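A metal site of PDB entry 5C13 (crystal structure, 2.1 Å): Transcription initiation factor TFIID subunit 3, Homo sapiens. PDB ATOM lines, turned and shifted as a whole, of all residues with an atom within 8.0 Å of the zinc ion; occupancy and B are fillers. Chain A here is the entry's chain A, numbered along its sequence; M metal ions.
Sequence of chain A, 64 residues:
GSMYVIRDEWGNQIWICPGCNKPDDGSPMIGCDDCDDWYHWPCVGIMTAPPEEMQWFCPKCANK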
ATOM      1  N   GLY A  31      18.795  -1.217 -16.167  1.00  0.00           N
ATOM      2  CA  GLY A  31      19.161  -2.498 -15.613  1.00  0.00           C
ATOM      3  C   GLY A  31      18.308  -3.638 -16.141  1.00  0.00           C
ATOM      4  O   GLY A  31      17.096  -3.506 -16.251  1.00  0.00           O
ATOM      5  N   CYS A  32      18.961  -4.750 -16.471  1.00  0.00           N
ATOM      6  CA  CYS A  32      18.267  -5.977 -16.885  1.00  0.00           C
ATOM      7  C   CYS A  32      17.476  -6.605 -15.728  1.00  0.00           C
ATOM      8  O   CYS A  32      18.000  -6.814 -14.644  1.00  0.00           O
ATOM      9  CB  CYS A  32      19.251  -7.003 -17.423  1.00  0.00           C
ATOM     10  SG  CYS A  32      18.410  -8.509 -18.048  1.00  0.00           S
ATOM     11  N   ASP A  33      16.212  -6.921 -15.973  1.00  0.00           N
ATOM     12  CA  ASP A  33      15.355  -7.473 -14.917  1.00  0.00           C
ATOM     13  C   ASP A  33      15.479  -8.979 -14.786  1.00  0.00           C
ATOM     14  O   ASP A  33      14.806  -9.587 -13.971  1.00  0.00           O
ATOM     15  CB  ASP A  33      13.907  -7.076 -15.178  1.00  0.00           C
ATOM     16  CG  ASP A  33      13.674  -5.599 -14.940  1.00  0.00           C
ATOM     17  OD1 ASP A  33      14.114  -5.080 -13.897  1.00  0.00           O
ATOM     18  OD2 ASP A  33      13.097  -4.931 -15.815  1.00  0.00           O
ATOM     19  N   ASP A  34      16.366  -9.560 -15.589  1.00  0.00           N
ATOM     20  CA  ASP A  34      16.747 -10.970 -15.437  1.00  0.00           C
ATOM     21  C   ASP A  34      18.132 -11.114 -14.757  1.00  0.00           C
ATOM     22  O   ASP A  34      18.229 -11.631 -13.648  1.00  0.00           O
ATOM     23  CB  ASP A  34      16.748 -11.654 -16.812  1.00  0.00           C
ATOM     24  CG  ASP A  34      16.995 -13.169 -16.729  1.00  0.00           C
ATOM     25  OD1 ASP A  34      17.307 -13.681 -15.626  1.00  0.00           O
ATOM     26  OD2 ASP A  34      16.888 -13.836 -17.776  1.00  0.00           O
ATOM     27  N   CYS A  35      19.191 -10.652 -15.416  1.00  0.00           N
ATOM     28  CA  CYS A  35      20.565 -10.853 -14.914  1.00  0.00           C
ATOM     29  C   CYS A  35      21.107  -9.648 -14.144  1.00  0.00           C
ATOM     30  O   CYS A  35      22.140  -9.728 -13.471  1.00  0.00           O
ATOM     31  CB  CYS A  35      21.494 -11.176 -16.085  1.00  0.00           C
ATOM     32  SG  CYS A  35      21.806  -9.762 -17.152  1.00  0.00           S
ATOM     33  N   ASP A  36      20.431  -8.525 -14.256  1.00  0.00           N
ATOM     34  CA  ASP A  36      20.782  -7.321 -13.535  1.00  0.00           C
ATOM     35  C   ASP A  36      22.115  -6.708 -13.931  1.00  0.00           C
ATOM     36  O   ASP A  36      22.700  -5.939 -13.150  1.00  0.00           O
ATOM     37  CB  ASP A  36      20.783  -7.604 -12.025  1.00  0.00           C
ATOM     38  CG  ASP A  36      20.547  -6.361 -11.213  1.00  0.00           C
ATOM     39  OD1 ASP A  36      20.049  -5.353 -11.768  1.00  0.00           O
ATOM     40  OD2 ASP A  36      20.837  -6.420  -9.998  1.00  0.00           O
ATOM     41  N   ASP A  37      22.603  -7.049 -15.127  1.00  0.00           N
ATOM     42  CA  ASP A  37      23.614  -6.246 -15.806  1.00  0.00           C
ATOM     43  C   ASP A  37      22.988  -4.922 -16.220  1.00  0.00           C
ATOM     44  O   ASP A  37      21.837  -4.907 -16.641  1.00  0.00           O
ATOM     45  CB  ASP A  37      24.141  -6.943 -17.053  1.00  0.00           C
ATOM     46  CG  ASP A  37      25.140  -8.034 -16.753  1.00  0.00           C
ATOM     47  OD1 ASP A  37      25.544  -8.195 -15.569  1.00  0.00           O
ATOM     48  OD2 ASP A  37      25.564  -8.703 -17.717  1.00  0.00           O
ATOM     49  N   TRP A  38      23.730  -3.832 -16.089  1.00  0.00           N
ATOM     50  CA  TRP A  38      23.294  -2.503 -16.471  1.00  0.00           C
ATOM     51  C   TRP A  38      24.019  -1.995 -17.716  1.00  0.00           C
ATOM     52  O   TRP A  38      25.220  -2.239 -17.868  1.00  0.00           O
ATOM     53  CB  TRP A  38      23.512  -1.539 -15.312  1.00  0.00           C
ATOM     54  CG  TRP A  38      22.594  -1.805 -14.126  1.00  0.00           C
ATOM     55  CD1 TRP A  38      22.621  -2.903 -13.321  1.00  0.00           C
ATOM     56  CD2 TRP A  38      21.525  -0.969 -13.638  1.00  0.00           C
ATOM     57  NE1 TRP A  38      21.626  -2.789 -12.346  1.00  0.00           N
ATOM     58  CE2 TRP A  38      20.963  -1.616 -12.533  1.00  0.00           C
ATOM     59  CE3 TRP A  38      21.015   0.274 -14.021  1.00  0.00           C
ATOM     60  CZ2 TRP A  38      19.891  -1.074 -11.809  1.00  0.00           C
ATOM     61  CZ3 TRP A  38      19.961   0.795 -13.313  1.00  0.00           C
ATOM     62  CH2 TRP A  38      19.415   0.118 -12.220  1.00  0.00           C
ATOM     63  N   TYR A  39      23.295  -1.295 -18.591  1.00  0.00           N
ATOM     64  CA  TYR A  39      23.846  -0.786 -19.856  1.00  0.00           C
ATOM     65  C   TYR A  39      23.514   0.655 -19.984  1.00  0.00           C
ATOM     66  O   TYR A  39      22.493   1.089 -19.486  1.00  0.00           O
ATOM     67  CB  TYR A  39      23.242  -1.512 -21.081  1.00  0.00           C
ATOM     68  CG  TYR A  39      23.622  -2.937 -21.265  1.00  0.00           C
ATOM     69  CD1 TYR A  39      23.172  -3.933 -20.411  1.00  0.00           C
ATOM     70  CD2 TYR A  39      24.405  -3.307 -22.349  1.00  0.00           C
ATOM     71  CE1 TYR A  39      23.539  -5.275 -20.610  1.00  0.00           C
ATOM     72  CE2 TYR A  39      24.743  -4.625 -22.572  1.00  0.00           C
ATOM     73  CZ  TYR A  39      24.348  -5.603 -21.696  1.00  0.00           C
ATOM     74  OH  TYR A  39      24.741  -6.905 -21.968  1.00  0.00           O
ATOM     75  N   TRP A  56      12.750  -4.182 -18.631  1.00  0.00           N
ATOM     76  CA  TRP A  56      13.696  -4.292 -19.737  1.00  0.00           C
ATOM     77  C   TRP A  56      14.643  -5.485 -19.553  1.00  0.00           C
ATOM     78  O   TRP A  56      14.900  -5.877 -18.422  1.00  0.00           O
ATOM     79  CB  TRP A  56      14.485  -3.013 -19.845  1.00  0.00           C
ATOM     80  CG  TRP A  56      15.488  -3.077 -20.942  1.00  0.00           C
ATOM     81  CD1 TRP A  56      15.268  -2.918 -22.282  1.00  0.00           C
ATOM     82  CD2 TRP A  56      16.886  -3.320 -20.782  1.00  0.00           C
ATOM     83  NE1 TRP A  56      16.456  -3.044 -22.971  1.00  0.00           N
ATOM     84  CE2 TRP A  56      17.460  -3.282 -22.062  1.00  0.00           C
ATOM     85  CE3 TRP A  56      17.705  -3.542 -19.667  1.00  0.00           C
ATOM     86  CZ2 TRP A  56      18.819  -3.473 -22.266  1.00  0.00           C
ATOM     87  CZ3 TRP A  56      19.050  -3.740 -19.865  1.00  0.00           C
ATOM     88  CH2 TRP A  56      19.602  -3.694 -21.153  1.00  0.00           C
ATOM     89  N   PHE A  57      15.180  -6.032 -20.661  1.00  0.00           N
ATOM     90  CA  PHE A  57      15.895  -7.333 -20.585  1.00  0.00           C
ATOM     91  C   PHE A  57      17.303  -7.553 -21.190  1.00  0.00           C
ATOM     92  O   PHE A  57      17.929  -8.559 -20.857  1.00  0.00           O
ATOM     93  CB  PHE A  57      14.955  -8.395 -21.146  1.00  0.00           C
ATOM     94  CG  PHE A  57      13.973  -8.874 -20.139  1.00  0.00           C
ATOM     95  CD1 PHE A  57      14.378  -9.733 -19.131  1.00  0.00           C
ATOM     96  CD2 PHE A  57      12.685  -8.400 -20.121  1.00  0.00           C
ATOM     97  CE1 PHE A  57      13.507 -10.152 -18.148  1.00  0.00           C
ATOM     98  CE2 PHE A  57      11.801  -8.809 -19.140  1.00  0.00           C
ATOM     99  CZ  PHE A  57      12.209  -9.678 -18.152  1.00  0.00           C
ATOM    100  N   CYS A  58      17.866  -6.674 -21.996  1.00  0.00           N
ATOM    101  CA  CYS A  58      19.264  -6.884 -22.428  1.00  0.00           C
ATOM    102  C   CYS A  58      19.376  -8.032 -23.444  1.00  0.00           C
ATOM    103  O   CYS A  58      18.683  -9.046 -23.334  1.00  0.00           O
ATOM    104  CB  CYS A  58      20.218  -7.136 -21.224  1.00  0.00           C
ATOM    105  SG  CYS A  58      20.994  -8.803 -20.974  1.00  0.00           S
ATOM    106  N   PRO A  59      20.242  -7.874 -24.456  1.00  0.00           N
ATOM    107  CA  PRO A  59      20.352  -8.864 -25.535  1.00  0.00           C
ATOM    108  C   PRO A  59      20.425 -10.307 -25.069  1.00  0.00           C
ATOM    109  O   PRO A  59      19.680 -11.157 -25.568  1.00  0.00           O
ATOM    110  CB  PRO A  59      21.652  -8.449 -26.234  1.00  0.00           C
ATOM    111  CG  PRO A  59      21.675  -6.983 -26.072  1.00  0.00           C
ATOM    112  CD  PRO A  59      21.154  -6.743 -24.661  1.00  0.00           C
ATOM    113  N   LYS A  60      21.273 -10.583 -24.099  1.00  0.00           N
ATOM    114  CA  LYS A  60      21.456 -11.959 -23.620  1.00  0.00           C
ATOM    115  C   LYS A  60      20.170 -12.579 -23.035  1.00  0.00           C
ATOM    116  O   LYS A  60      19.912 -13.750 -23.308  1.00  0.00           O
ATOM    117  CB  LYS A  60      22.601 -12.002 -22.599  1.00  0.00           C
ATOM    118  CG  LYS A  60      23.924 -11.524 -23.214  1.00  0.00           C
ATOM    119  CD  LYS A  60      25.011 -11.327 -22.193  1.00  0.00           C
ATOM    120  CE  LYS A  60      26.298 -10.785 -22.819  1.00  0.00           C
ATOM    121  NZ  LYS A  60      26.893  -9.671 -21.980  1.00  0.00           N
ATOM    122  N   CYS A  61      19.345 -11.834 -22.301  1.00  0.00           N
ATOM    123  CA  CYS A  61      18.234 -12.485 -21.578  1.00  0.00           C
ATOM    124  C   CYS A  61      16.878 -12.482 -22.311  1.00  0.00           C
ATOM    125  O   CYS A  61      16.540 -11.570 -23.076  1.00  0.00           O
ATOM    126  CB  CYS A  61      18.073 -11.848 -20.184  1.00  0.00           C
ATOM    127  SG  CYS A  61      19.552 -12.008 -19.128  1.00  0.00           S
HETATM  128 ZN    ZN M   1      20.321  -9.733 -18.814  1.00  0.00          ZN
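SG of Cys 35 lies close to N of Asp 37 (3.5 Å).
SG of Cys 32 sits close to O of Phe 57 (2.9 Å).
The backbone NH of Cys 32 is in hydrogen-bond range of the backbone carbonyl oxygen of Asp 37 (2.9 Å).
The side-chain sulfur of Cys 61 lies close to the side-chain carboxylate of Asp 34, 3.5 Å away.
SG of Cys 32 lies close to N of Asp 34 (3.4 Å).
The backbone NH of Lys 60 sits close to the side-chain sulfur of Cys 58, 3.6 Å away.
The zinc ion is bound by SG of Cys 35 (2.2 Å), SG of Cys 32 (2.4 Å), SG of Cys 61 (2.4 Å) and SG of Cys 58 (2.4 Å).
Residues that only touch the zinc ion: Phe 57.
The nearest printed residue that does not touch the zinc ion is Asp 34 (4.5 Å).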
